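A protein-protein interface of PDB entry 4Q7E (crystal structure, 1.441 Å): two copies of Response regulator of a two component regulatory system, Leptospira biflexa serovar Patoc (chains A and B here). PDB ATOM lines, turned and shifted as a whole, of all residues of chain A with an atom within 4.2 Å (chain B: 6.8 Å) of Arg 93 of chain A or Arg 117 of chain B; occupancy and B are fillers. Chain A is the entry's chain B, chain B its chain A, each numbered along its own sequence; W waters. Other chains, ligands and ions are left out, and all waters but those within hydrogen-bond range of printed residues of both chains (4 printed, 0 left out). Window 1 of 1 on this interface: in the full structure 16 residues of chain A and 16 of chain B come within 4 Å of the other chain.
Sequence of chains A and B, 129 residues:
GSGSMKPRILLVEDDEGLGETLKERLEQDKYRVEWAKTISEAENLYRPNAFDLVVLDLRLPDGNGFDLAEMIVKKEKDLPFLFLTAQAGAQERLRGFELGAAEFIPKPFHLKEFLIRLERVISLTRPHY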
ATOM      1  N   ALA A  88      -7.597  23.320  12.055  1.00  0.00           N
ATOM      2  CA  ALA A  88      -8.903  23.040  11.472  1.00  0.00           C
ATOM      3  C   ALA A  88      -9.723  22.062  12.297  1.00  0.00           C
ATOM      4  O   ALA A  88     -10.627  21.393  11.770  1.00  0.00           O
ATOM      5  CB  ALA A  88      -8.728  22.530  10.029  1.00  0.00           C
ATOM      6  N   GLY A  89      -9.485  22.035  13.597  1.00  0.00           N
ATOM      7  CA  GLY A  89     -10.243  21.138  14.469  1.00  0.00           C
ATOM      8  C   GLY A  89     -11.643  21.609  14.769  1.00  0.00           C
ATOM      9  O   GLY A  89     -12.084  22.706  14.366  1.00  0.00           O
ATOM     10  N   ALA A  90     -12.369  20.758  15.479  1.00  0.00           N
ATOM     11  CA  ALA A  90     -13.804  20.975  15.699  1.00  0.00           C
ATOM     12  C   ALA A  90     -14.115  22.287  16.387  1.00  0.00           C
ATOM     13  O   ALA A  90     -15.060  22.974  15.996  1.00  0.00           O
ATOM     14  CB  ALA A  90     -14.437  19.798  16.465  1.00  0.00           C
ATOM     15  N   GLN A  91     -13.291  22.661  17.380  1.00  0.00           N
ATOM     16  CA  GLN A  91     -13.552  23.885  18.125  1.00  0.00           C
ATOM     17  C   GLN A  91     -13.381  25.120  17.223  1.00  0.00           C
ATOM     18  O   GLN A  91     -14.202  26.025  17.225  1.00  0.00           O
ATOM     19  CB  GLN A  91     -12.574  23.983  19.297  1.00  0.00           C
ATOM     20  CG  GLN A  91     -12.684  25.239  20.112  1.00  0.00           C
ATOM     21  CD  GLN A  91     -11.819  25.117  21.334  1.00  0.00           C
ATOM     22  OE1 GLN A  91     -11.880  24.107  22.042  1.00  0.00           O
ATOM     23  NE2 GLN A  91     -10.941  26.094  21.542  1.00  0.00           N
ATOM     24  N   GLU A  92     -12.324  25.117  16.440  1.00  0.00           N
ATOM     25  CA  GLU A  92     -12.014  26.257  15.587  1.00  0.00           C
ATOM     26  C   GLU A  92     -13.036  26.378  14.477  1.00  0.00           C
ATOM     27  O   GLU A  92     -13.468  27.497  14.157  1.00  0.00           O
ATOM     28  CB  GLU A  92     -10.614  26.130  14.992  1.00  0.00           C
ATOM     29  CG  GLU A  92      -9.482  26.282  15.996  1.00  0.00           C
ATOM     30  CD  GLU A  92      -9.064  25.009  16.720  1.00  0.00           C
ATOM     31  OE1 GLU A  92      -9.737  23.968  16.620  1.00  0.00           O
ATOM     32  OE2 GLU A  92      -8.031  25.067  17.421  1.00  0.00           O
ATOM     33  N   ARG A  93     -13.453  25.250  13.910  1.00  0.00           N
ATOM     34  CA  ARG A  93     -14.473  25.331  12.869  1.00  0.00           C
ATOM     35  C   ARG A  93     -15.787  25.847  13.436  1.00  0.00           C
ATOM     36  O   ARG A  93     -16.453  26.695  12.822  1.00  0.00           O
ATOM     37  CB  ARG A  93     -14.677  23.978  12.223  1.00  0.00           C
ATOM     38  CG  ARG A  93     -13.413  23.479  11.469  1.00  0.00           C
ATOM     39  CD  ARG A  93     -13.778  22.386  10.458  1.00  0.00           C
ATOM     40  NE  ARG A  93     -14.759  21.458  11.027  1.00  0.00           N
ATOM     41  CZ  ARG A  93     -14.455  20.424  11.807  1.00  0.00           C
ATOM     42  NH1 ARG A  93     -13.192  20.130  12.074  1.00  0.00           N
ATOM     43  NH2 ARG A  93     -15.429  19.715  12.337  1.00  0.00           N
ATOM     44  N   LEU A  94     -16.162  25.351  14.615  1.00  0.00           N
ATOM     45  CA  LEU A  94     -17.402  25.850  15.232  1.00  0.00           C
ATOM     46  C   LEU A  94     -17.334  27.351  15.447  1.00  0.00           C
ATOM     47  O   LEU A  94     -18.260  28.057  15.099  1.00  0.00           O
ATOM     48  CB  LEU A  94     -17.755  25.134  16.532  1.00  0.00           C
ATOM     49  CG  LEU A  94     -18.983  25.668  17.289  1.00  0.00           C
ATOM     50  CD1 LEU A  94     -20.271  25.506  16.463  1.00  0.00           C
ATOM     51  CD2 LEU A  94     -19.081  24.979  18.649  1.00  0.00           C
ATOM     52  N   ARG A  95     -16.215  27.831  15.987  1.00  0.00           N
ATOM     53  CA  ARG A  95     -16.040  29.252  16.239  1.00  0.00           C
ATOM     54  C   ARG A  95     -16.098  30.040  14.937  1.00  0.00           C
ATOM     55  O   ARG A  95     -16.760  31.067  14.865  1.00  0.00           O
ATOM     56  CB  ARG A  95     -14.715  29.488  16.973  1.00  0.00           C
ATOM     57  CG  ARG A  95     -14.511  30.949  17.365  1.00  0.00           C
ATOM     58  CD  ARG A  95     -13.163  31.192  18.021  1.00  0.00           C
ATOM     59  NE  ARG A  95     -13.018  32.628  18.186  1.00  0.00           N
ATOM     60  CZ  ARG A  95     -12.000  33.198  18.811  1.00  0.00           C
ATOM     61  NH1 ARG A  95     -11.074  32.429  19.341  1.00  0.00           N
ATOM     62  NH2 ARG A  95     -11.926  34.512  18.923  1.00  0.00           N
ATOM     63  N   GLY A  96     -15.430  29.541  13.898  1.00  0.00           N
ATOM     64  CA  GLY A  96     -15.438  30.206  12.618  1.00  0.00           C
ATOM     65  C   GLY A  96     -16.815  30.307  11.961  1.00  0.00           C
ATOM     66  O   GLY A  96     -17.206  31.389  11.498  1.00  0.00           O
ATOM     67  N   PHE A  97     -17.557  29.185  11.932  1.00  0.00           N
ATOM     68  CA  PHE A  97     -18.905  29.204  11.361  1.00  0.00           C
ATOM     69  C   PHE A  97     -19.881  30.035  12.203  1.00  0.00           C
ATOM     70  O   PHE A  97     -20.732  30.740  11.652  1.00  0.00           O
ATOM     71  CB  PHE A  97     -19.425  27.785  11.086  1.00  0.00           C
ATOM     72  CG  PHE A  97     -18.780  27.158   9.871  1.00  0.00           C
ATOM     73  CD1 PHE A  97     -19.182  27.525   8.598  1.00  0.00           C
ATOM     74  CD2 PHE A  97     -17.794  26.181   9.992  1.00  0.00           C
ATOM     75  CE1 PHE A  97     -18.581  26.982   7.475  1.00  0.00           C
ATOM     76  CE2 PHE A  97     -17.193  25.626   8.877  1.00  0.00           C
ATOM     77  CZ  PHE A  97     -17.584  26.012   7.593  1.00  0.00           C
ATOM     78  N   PHE A 104     -14.411  26.988   5.314  1.00  0.00           N
ATOM     79  CA  PHE A 104     -13.346  26.589   6.230  1.00  0.00           C
ATOM     80  C   PHE A 104     -12.656  25.419   5.537  1.00  0.00           C
ATOM     81  O   PHE A 104     -13.217  24.334   5.416  1.00  0.00           O
ATOM     82  CB  PHE A 104     -13.892  26.232   7.626  1.00  0.00           C
ATOM     83  CG  PHE A 104     -12.859  26.292   8.706  1.00  0.00           C
ATOM     84  CD1 PHE A 104     -11.711  25.490   8.620  1.00  0.00           C
ATOM     85  CD2 PHE A 104     -13.012  27.133   9.810  1.00  0.00           C
ATOM     86  CE1 PHE A 104     -10.735  25.572   9.583  1.00  0.00           C
ATOM     87  CE2 PHE A 104     -12.025  27.198  10.772  1.00  0.00           C
ATOM     88  CZ  PHE A 104     -10.896  26.418  10.660  1.00  0.00           C
ATOM     89  N   ARG A 117     -13.982  25.193  -4.119  1.00  0.00           N
ATOM     90  CA  ARG A 117     -14.689  25.762  -2.987  1.00  0.00           C
ATOM     91  C   ARG A 117     -14.751  27.292  -3.022  1.00  0.00           C
ATOM     92  O   ARG A 117     -15.795  27.863  -2.692  1.00  0.00           O
ATOM     93  CB  ARG A 117     -14.084  25.229  -1.690  1.00  0.00           C
ATOM     94  CG  ARG A 117     -14.280  23.682  -1.541  1.00  0.00           C
ATOM     95  CD  ARG A 117     -13.537  23.077  -0.322  1.00  0.00           C
ATOM     96  NE  ARG A 117     -14.281  23.354   0.905  1.00  0.00           N
ATOM     97  CZ  ARG A 117     -14.113  22.682   2.034  1.00  0.00           C
ATOM     98  NH1 ARG A 117     -13.182  21.713   2.111  1.00  0.00           N
ATOM     99  NH2 ARG A 117     -14.891  22.960   3.059  1.00  0.00           N
ATOM    100  N   LEU B  82     -23.835  15.518   0.598  1.00  0.00           N
ATOM    101  CA  LEU B  82     -22.632  15.906   1.301  1.00  0.00           C
ATOM    102  C   LEU B  82     -22.056  14.775   2.104  1.00  0.00           C
ATOM    103  O   LEU B  82     -22.801  13.855   2.538  1.00  0.00           O
ATOM    104  CB  LEU B  82     -22.877  17.145   2.158  1.00  0.00           C
ATOM    105  CG  LEU B  82     -23.797  17.035   3.368  1.00  0.00           C
ATOM    106  CD1 LEU B  82     -23.030  16.514   4.605  1.00  0.00           C
ATOM    107  CD2 LEU B  82     -24.472  18.356   3.693  1.00  0.00           C
ATOM    108  N   PHE B  97     -15.412  16.602  -3.807  1.00  0.00           N
ATOM    109  CA  PHE B  97     -15.714  17.853  -4.520  1.00  0.00           C
ATOM    110  C   PHE B  97     -15.721  17.683  -6.032  1.00  0.00           C
ATOM    111  O   PHE B  97     -16.588  18.253  -6.679  1.00  0.00           O
ATOM    112  CB  PHE B  97     -14.833  19.013  -4.038  1.00  0.00           C
ATOM    113  CG  PHE B  97     -15.257  19.564  -2.679  1.00  0.00           C
ATOM    114  CD1 PHE B  97     -16.431  20.333  -2.547  1.00  0.00           C
ATOM    115  CD2 PHE B  97     -14.507  19.309  -1.533  1.00  0.00           C
ATOM    116  CE1 PHE B  97     -16.830  20.828  -1.299  1.00  0.00           C
ATOM    117  CE2 PHE B  97     -14.918  19.775  -0.286  1.00  0.00           C
ATOM    118  CZ  PHE B  97     -16.083  20.521  -0.157  1.00  0.00           C
ATOM    119  N   ALA B 102     -21.898  18.723  -2.345  1.00  0.00           N
ATOM    120  CA  ALA B 102     -22.333  20.026  -1.923  1.00  0.00           C
ATOM    121  C   ALA B 102     -21.562  20.522  -0.700  1.00  0.00           C
ATOM    122  O   ALA B 102     -21.565  21.699  -0.408  1.00  0.00           O
ATOM    123  CB  ALA B 102     -23.833  20.020  -1.646  1.00  0.00           C
ATOM    124  N   GLU B 103     -20.946  19.606   0.024  1.00  0.00           N
ATOM    125  CA  GLU B 103     -20.249  19.926   1.254  1.00  0.00           C
ATOM    126  C   GLU B 103     -19.419  18.723   1.660  1.00  0.00           C
ATOM    127  O   GLU B 103     -19.644  17.586   1.192  1.00  0.00           O
ATOM    128  CB  GLU B 103     -21.223  20.305   2.379  1.00  0.00           C
ATOM    129  CG  GLU B 103     -21.284  21.779   2.793  1.00  0.00           C
ATOM    130  CD  GLU B 103     -20.034  22.280   3.530  1.00  0.00           C
ATOM    131  OE1 GLU B 103     -18.921  21.711   3.375  1.00  0.00           O
ATOM    132  OE2 GLU B 103     -20.216  23.285   4.244  1.00  0.00           O
ATOM    133  N   PHE B 104     -18.463  18.960   2.549  1.00  0.00           N
ATOM    134  CA  PHE B 104     -17.617  17.908   3.089  1.00  0.00           C
ATOM    135  C   PHE B 104     -17.295  18.334   4.505  1.00  0.00           C
ATOM    136  O   PHE B 104     -16.544  19.287   4.707  1.00  0.00           O
ATOM    137  CB  PHE B 104     -16.354  17.701   2.223  1.00  0.00           C
ATOM    138  CG  PHE B 104     -15.710  16.358   2.414  1.00  0.00           C
ATOM    139  CD1 PHE B 104     -15.236  15.973   3.671  1.00  0.00           C
ATOM    140  CD2 PHE B 104     -15.654  15.446   1.368  1.00  0.00           C
ATOM    141  CE1 PHE B 104     -14.672  14.734   3.858  1.00  0.00           C
ATOM    142  CE2 PHE B 104     -15.091  14.173   1.549  1.00  0.00           C
ATOM    143  CZ  PHE B 104     -14.586  13.821   2.782  1.00  0.00           C
ATOM    144  N   ILE B 105     -17.895  17.638   5.476  1.00  0.00           N
ATOM    145  CA  ILE B 105     -17.792  18.013   6.872  1.00  0.00           C
ATOM    146  C   ILE B 105     -17.069  16.887   7.584  1.00  0.00           C
ATOM    147  O   ILE B 105     -17.537  15.748   7.549  1.00  0.00           O
ATOM    148  CB  ILE B 105     -19.187  18.224   7.484  1.00  0.00           C
ATOM    149  CG1 ILE B 105     -19.989  19.266   6.680  1.00  0.00           C
ATOM    150  CG2 ILE B 105     -19.107  18.605   8.987  1.00  0.00           C
ATOM    151  CD1 ILE B 105     -21.484  19.434   7.091  1.00  0.00           C
ATOM    152  N   PRO B 106     -15.962  17.184   8.273  1.00  0.00           N
ATOM    153  CA  PRO B 106     -15.223  16.109   8.961  1.00  0.00           C
ATOM    154  C   PRO B 106     -15.856  15.713  10.287  1.00  0.00           C
ATOM    155  O   PRO B 106     -16.565  16.501  10.941  1.00  0.00           O
ATOM    156  CB  PRO B 106     -13.858  16.724   9.229  1.00  0.00           C
ATOM    157  CG  PRO B 106     -14.195  18.240   9.395  1.00  0.00           C
ATOM    158  CD  PRO B 106     -15.338  18.516   8.439  1.00  0.00           C
ATOM    159  N   LYS B 107     -15.579  14.467  10.678  1.00  0.00           N
ATOM    160  CA  LYS B 107     -15.710  14.060  12.079  1.00  0.00           C
ATOM    161  C   LYS B 107     -14.318  14.111  12.696  1.00  0.00           C
ATOM    162  O   LYS B 107     -13.347  13.722  12.052  1.00  0.00           O
ATOM    163  CB  LYS B 107     -16.256  12.633  12.135  1.00  0.00           C
ATOM    164  CG  LYS B 107     -17.672  12.435  11.585  1.00  0.00           C
ATOM    165  CD  LYS B 107     -18.049  10.961  11.657  1.00  0.00           C
ATOM    166  CE  LYS B 107     -19.448  10.702  10.989  1.00  0.00           C
ATOM    167  NZ  LYS B 107     -19.756   9.214  11.037  1.00  0.00           N
ATOM    168  N   PRO B 108     -14.198  14.562  13.954  1.00  0.00           N
ATOM    169  CA  PRO B 108     -15.296  14.968  14.800  1.00  0.00           C
ATOM    170  C   PRO B 108     -15.825  16.353  14.490  1.00  0.00           C
ATOM    171  O   PRO B 108     -15.113  17.215  13.925  1.00  0.00           O
ATOM    172  CB  PRO B 108     -14.667  14.940  16.208  1.00  0.00           C
ATOM    173  CG  PRO B 108     -13.231  15.310  15.938  1.00  0.00           C
ATOM    174  CD  PRO B 108     -12.910  14.586  14.668  1.00  0.00           C
ATOM    175  N   PHE B 109     -17.045  16.605  14.928  1.00  0.00           N
ATOM    176  CA  PHE B 109     -17.696  17.893  14.718  1.00  0.00           C
ATOM    177  C   PHE B 109     -18.656  18.188  15.863  1.00  0.00           C
ATOM    178  O   PHE B 109     -19.280  17.275  16.435  1.00  0.00           O
ATOM    179  CB  PHE B 109     -18.455  17.909  13.372  1.00  0.00           C
ATOM    180  CG  PHE B 109     -19.654  16.981  13.359  1.00  0.00           C
ATOM    181  CD1 PHE B 109     -19.479  15.621  13.148  1.00  0.00           C
ATOM    182  CD2 PHE B 109     -20.933  17.464  13.604  1.00  0.00           C
ATOM    183  CE1 PHE B 109     -20.546  14.740  13.184  1.00  0.00           C
ATOM    184  CE2 PHE B 109     -22.023  16.573  13.632  1.00  0.00           C
ATOM    185  CZ  PHE B 109     -21.819  15.219  13.414  1.00  0.00           C
ATOM    186  N   HIS B 110     -18.866  19.467  16.139  1.00  0.00           N
ATOM    187  CA  HIS B 110     -19.958  19.893  17.001  1.00  0.00           C
ATOM    188  C   HIS B 110     -21.243  20.018  16.208  1.00  0.00           C
ATOM    189  O   HIS B 110     -21.234  20.502  15.085  1.00  0.00           O
ATOM    190  CB  HIS B 110     -19.589  21.217  17.664  1.00  0.00           C
ATOM    191  CG  HIS B 110     -18.427  21.098  18.582  1.00  0.00           C
ATOM    192  ND1 HIS B 110     -18.494  20.407  19.784  1.00  0.00           N
ATOM    193  CD2 HIS B 110     -17.154  21.535  18.467  1.00  0.00           C
ATOM    194  CE1 HIS B 110     -17.306  20.450  20.366  1.00  0.00           C
ATOM    195  NE2 HIS B 110     -16.483  21.148  19.603  1.00  0.00           N
ATOM    196  N   LYS B 112     -23.718  22.003  16.211  1.00  0.00           N
ATOM    197  CA  LYS B 112     -24.096  23.320  15.694  1.00  0.00           C
ATOM    198  C   LYS B 112     -23.344  23.720  14.427  1.00  0.00           C
ATOM    199  O   LYS B 112     -23.902  24.417  13.564  1.00  0.00           O
ATOM    200  CB  LYS B 112     -24.010  24.363  16.801  1.00  0.00           C
ATOM    201  CG  LYS B 112     -25.227  24.211  17.727  1.00  0.00           C
ATOM    202  CD  LYS B 112     -25.352  25.278  18.754  1.00  0.00           C
ATOM    203  CE  LYS B 112     -26.545  24.983  19.677  1.00  0.00           C
ATOM    204  NZ  LYS B 112     -26.974  26.152  20.467  1.00  0.00           N
ATOM    205  N   GLU B 113     -22.114  23.232  14.284  1.00  0.00           N
ATOM    206  CA  GLU B 113     -21.362  23.448  13.042  1.00  0.00           C
ATOM    207  C   GLU B 113     -22.055  22.757  11.890  1.00  0.00           C
ATOM    208  O   GLU B 113     -22.251  23.335  10.806  1.00  0.00           O
ATOM    209  CB  GLU B 113     -19.933  22.934  13.145  1.00  0.00           C
ATOM    210  CG  GLU B 113     -19.158  23.205  11.870  1.00  0.00           C
ATOM    211  CD  GLU B 113     -18.026  22.245  11.599  1.00  0.00           C
ATOM    212  OE1 GLU B 113     -17.747  21.344  12.411  1.00  0.00           O
ATOM    213  OE2 GLU B 113     -17.383  22.402  10.541  1.00  0.00           O
ATOM    214  N   PHE B 114     -22.417  21.501  12.130  1.00  0.00           N
ATOM    215  CA  PHE B 114     -23.145  20.718  11.119  1.00  0.00           C
ATOM    216  C   PHE B 114     -24.450  21.418  10.713  1.00  0.00           C
ATOM    217  O   PHE B 114     -24.761  21.518   9.515  1.00  0.00           O
ATOM    218  CB  PHE B 114     -23.411  19.292  11.654  1.00  0.00           C
ATOM    219  CG  PHE B 114     -24.281  18.458  10.792  1.00  0.00           C
ATOM    220  CD1 PHE B 114     -23.755  17.800   9.705  1.00  0.00           C
ATOM    221  CD2 PHE B 114     -25.623  18.306  11.080  1.00  0.00           C
ATOM    222  CE1 PHE B 114     -24.548  17.014   8.910  1.00  0.00           C
ATOM    223  CE2 PHE B 114     -26.432  17.522  10.279  1.00  0.00           C
ATOM    224  CZ  PHE B 114     -25.894  16.882   9.200  1.00  0.00           C
ATOM    225  N   LEU B 115     -25.194  21.936  11.691  1.00  0.00           N
ATOM    226  CA  LEU B 115     -26.453  22.611  11.388  1.00  0.00           C
ATOM    227  C   LEU B 115     -26.256  23.891  10.565  1.00  0.00           C
ATOM    228  O   LEU B 115     -27.012  24.161   9.635  1.00  0.00           O
ATOM    229  CB  LEU B 115     -27.260  22.908  12.659  1.00  0.00           C
ATOM    230  CG  LEU B 115     -27.737  21.653  13.406  1.00  0.00           C
ATOM    231  CD1 LEU B 115     -28.328  22.007  14.784  1.00  0.00           C
ATOM    232  CD2 LEU B 115     -28.712  20.804  12.584  1.00  0.00           C
ATOM    233  N   ILE B 116     -25.228  24.679  10.876  1.00  0.00           N
ATOM    234  CA  ILE B 116     -24.975  25.881  10.091  1.00  0.00           C
ATOM    235  C   ILE B 116     -24.661  25.499   8.642  1.00  0.00           C
ATOM    236  O   ILE B 116     -25.157  26.105   7.691  1.00  0.00           O
ATOM    237  CB  ILE B 116     -23.816  26.726  10.707  1.00  0.00           C
ATOM    238  CG1 ILE B 116     -24.283  27.405  12.025  1.00  0.00           C
ATOM    239  CG2 ILE B 116     -23.304  27.791   9.709  1.00  0.00           C
ATOM    240  CD1 ILE B 116     -23.147  27.895  12.853  1.00  0.00           C
ATOM    241  N   ARG B 117     -23.765  24.531   8.474  1.00  0.00           N
ATOM    242  CA  ARG B 117     -23.316  24.166   7.133  1.00  0.00           C
ATOM    243  C   ARG B 117     -24.448  23.529   6.339  1.00  0.00           C
ATOM    244  O   ARG B 117     -24.615  23.788   5.139  1.00  0.00           O
ATOM    245  CB  ARG B 117     -22.096  23.264   7.228  1.00  0.00           C
ATOM    246  CG  ARG B 117     -20.883  24.030   7.795  1.00  0.00           C
ATOM    247  CD  ARG B 117     -19.693  23.125   8.031  1.00  0.00           C
ATOM    248  NE  ARG B 117     -18.996  22.817   6.800  1.00  0.00           N
ATOM    249  CZ  ARG B 117     -17.709  22.440   6.714  1.00  0.00           C
ATOM    250  NH1 ARG B 117     -17.159  22.242   5.520  1.00  0.00           N
ATOM    251  NH2 ARG B 117     -16.958  22.244   7.821  1.00  0.00           N
ATOM    252  N   LEU B 118     -25.270  22.746   7.021  1.00  0.00           N
ATOM    253  CA  LEU B 118     -26.370  22.078   6.345  1.00  0.00           C
ATOM    254  C   LEU B 118     -27.465  23.081   5.935  1.00  0.00           C
ATOM    255  O   LEU B 118     -28.056  22.957   4.869  1.00  0.00           O
ATOM    256  CB  LEU B 118     -26.911  20.933   7.220  1.00  0.00           C
ATOM    257  CG  LEU B 118     -28.046  20.106   6.618  1.00  0.00           C
ATOM    258  CD1 LEU B 118     -28.017  18.654   7.077  1.00  0.00           C
ATOM    259  CD2 LEU B 118     -29.380  20.709   6.983  1.00  0.00           C
ATOM    260  N   GLU B 119     -27.732  24.085   6.770  1.00  0.00           N
ATOM    261  CA  GLU B 119     -28.713  25.088   6.425  1.00  0.00           C
ATOM    262  C   GLU B 119     -28.281  25.874   5.177  1.00  0.00           C
ATOM    263  O   GLU B 119     -29.112  26.167   4.319  1.00  0.00           O
ATOM    264  CB  GLU B 119     -28.987  25.978   7.646  1.00  0.00           C
ATOM    265  CG  GLU B 119     -29.966  27.108   7.467  1.00  0.00           C
ATOM    266  CD  GLU B 119     -30.052  27.995   8.723  1.00  0.00           C
ATOM    267  OE1 GLU B 119     -29.268  28.974   8.811  1.00  0.00           O
ATOM    268  OE2 GLU B 119     -30.875  27.710   9.632  1.00  0.00           O
ATOM    269  N   ARG B 120     -26.976  26.145   5.014  1.00  0.00           N
ATOM    270  CA  ARG B 120     -26.525  26.809   3.785  1.00  0.00           C
ATOM    271  C   ARG B 120     -26.692  25.904   2.569  1.00  0.00           C
ATOM    272  O   ARG B 120     -27.041  26.388   1.493  1.00  0.00           O
ATOM    273  CB  ARG B 120     -25.078  27.279   3.925  1.00  0.00           C
ATOM    274  CG  ARG B 120     -24.899  28.257   5.057  1.00  0.00           C
ATOM    275  CD  ARG B 120     -23.439  28.444   5.289  1.00  0.00           C
ATOM    276  NE  ARG B 120     -23.193  29.461   6.310  1.00  0.00           N
ATOM    277  CZ  ARG B 120     -21.961  29.851   6.627  1.00  0.00           C
ATOM    278  NH1 ARG B 120     -20.946  29.271   6.006  1.00  0.00           N
ATOM    279  NH2 ARG B 120     -21.735  30.786   7.552  1.00  0.00           N
ATOM    280  N   VAL B 121     -26.487  24.603   2.726  1.00  0.00           N
ATOM    281  CA  VAL B 121     -26.699  23.710   1.589  1.00  0.00           C
ATOM    282  C   VAL B 121     -28.184  23.698   1.197  1.00  0.00           C
ATOM    283  O   VAL B 121     -28.542  23.751   0.004  1.00  0.00           O
ATOM    284  CB  VAL B 121     -26.217  22.256   1.919  1.00  0.00           C
ATOM    285  CG1 VAL B 121     -26.728  21.258   0.852  1.00  0.00           C
ATOM    286  CG2 VAL B 121     -24.684  22.207   2.025  1.00  0.00           C
ATOM    287  N   ILE B 122     -29.070  23.662   2.188  1.00  0.00           N
ATOM    288  CA  ILE B 122     -30.496  23.716   1.895  1.00  0.00           C
ATOM    289  C   ILE B 122     -30.872  25.025   1.217  1.00  0.00           C
ATOM    290  O   ILE B 122     -31.681  25.026   0.295  1.00  0.00           O
ATOM    291  CB  ILE B 122     -31.329  23.459   3.180  1.00  0.00           C
ATOM    292  CG1 ILE B 122     -31.102  22.040   3.678  1.00  0.00           C
ATOM    293  CG2 ILE B 122     -32.848  23.739   2.967  1.00  0.00           C
ATOM    294  CD1 ILE B 122     -31.534  20.935   2.709  1.00  0.00           C
HETATM  295  O   HOH W   1     -12.487  17.632  13.379  1.00  0.00           O
HETATM  296  O   HOH W   2     -14.184  22.127   6.948  1.00  0.00           O
HETATM  297  O   HOH W   3     -17.415  21.673  15.049  1.00  0.00           O
HETATM  298  O   HOH W   4     -13.950  20.272   4.488  1.00  0.00           O
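Ala 90 of chain A touches Pro 108 of chain B. Ala 90 of chain A touches His 110 of chain B. Arg 93 of chain A touches Phe 109 of chain B. NH2 of Arg 117 of chain B touches NE of Arg 93 of chain A (3.97 Å). Leu 94 of chain A touches His 110 of chain B. Lys 112 of chain B touches Leu 94 of chain A (CB to CD1, 3.9 Å). Glu 113 of chain B touches Leu 94 of chain A (N to CD1, 3.6 Å). CD1 of Ile 116 of chain B touches O of Phe 97 of chain A, at 3.9 Å. Phe 97 of chain A touches Arg 117 of chain B. Arg 117 of chain A touches Phe 97 of chain B.
Water W3 lies within hydrogen-bond range of the side-chain carboxylate (OE1) of Glu 113 of chain B (2.7 Å), the backbone carbonyl oxygen (O) of Ala 90 of chain A (2.9 Å) and the backbone NH (N) of His 110 of chain B (2.9 Å). Water W1 bridges the backbone carbonyl oxygen (O) of Pro 108 of chain B (2.7 Å) and the guanidinium group (NH1) of Arg 93 of chain A (2.9 Å). Water W4 bridges the backbone carbonyl oxygen (O) of Phe 104 of chain B and the guanidinium group (NH1) of Arg 117 of chain A.
Arg 93 of chain A touches five residues of chain B. Printed residues of chain B within 4 Å of Phe 97 of chain A: Glu 113 (3.6 Å), Ile 116 (3.9 Å), Arg 117 (3.6 Å) and Arg 120 (3.6 Å). Phe 104 of chain A touches none of the printed residues of chain B. Of the printed residues of chain A, Pro 106 of chain B touches Arg 93. Lys 107 of chain B touches none of the printed residues of chain A. Of the printed residues of chain A, Pro 108 of chain B touches Ala 90 (3.7 Å) and Arg 93 (3.0 Å). Of the printed residues of chain A, Phe 109 of chain B touches Arg 93 (3.7 Å). Of the printed residues of chain A, Glu 113 of chain B touches Arg 93, Leu 94 and Phe 97. Arg 117 of chain B touches three residues of chain A. The nearest printed residue of chain B that does not touch Leu 94 of chain A is Ile 116 of chain B (5.2 Å).
OE2 of Glu 113 of chain B lies within salt-bridge range of NH2 of Arg 117 of chain B. OE1 of Glu 103 of chain B is in salt-bridge range of NH1 of Arg 117 of chain B (2.8 Å). The guanidinium group (NH2) of Arg 117 of chain A is in hydrogen-bond range of the backbone carbonyl oxygen (O) of Phe 104 of chain A. The backbone carbonyl oxygen (O) of Phe 104 of chain B sits at hydrogen-bond distance from the guanidinium group (NH1) of Arg 117 of chain B (3.1 Å). The guanidinium group (NH1) of Arg 93 of chain A lies within hydrogen-bond range of the backbone carbonyl oxygen (O) of Ala 88 of chain A (2.9 Å).
Phe 97 of chain A touches Arg 117 of chain B, and with the chains exchanged Arg 117 of chain A touches Phe 97 of chain B. Arg 117 of chain B touches its own counterpart, Arg 117 of chain A.
O of Pro 108 of chain B lies within hydrogen-bond range of NH2 of Arg 93 of chain A (3.0 Å). The guanidinium group (NH1) of Arg 117 of chain B lies close to the guanidinium group (NH2) of Arg 117 of chain A (3.4 Å). The side-chain carboxylate (OE2) of Glu 113 of chain B is in salt-bridge range of the guanidinium group (NE) of Arg 93 of chain A, at 2.8 Å.
Of the 22 printed residues of chain B, 10 touch a printed residue of chain A. Printed residues of chain B that touch a printed residue of chain A: Phe 97, Pro 106, Pro 108, Phe 109, His 110, Lys 112, Glu 113, Ile 116, Arg 117 and Arg 120. Hydrophobic or aromatic side chains of chain B within 4 Å of the printed part of chain A: Phe 97, Pro 106, Phe 109, His 110 and Ile 116. Hydrophobic or aromatic side chains of chain A within 4 Å of the printed part of chain B: Ala 90, Leu 94 and Phe 97.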
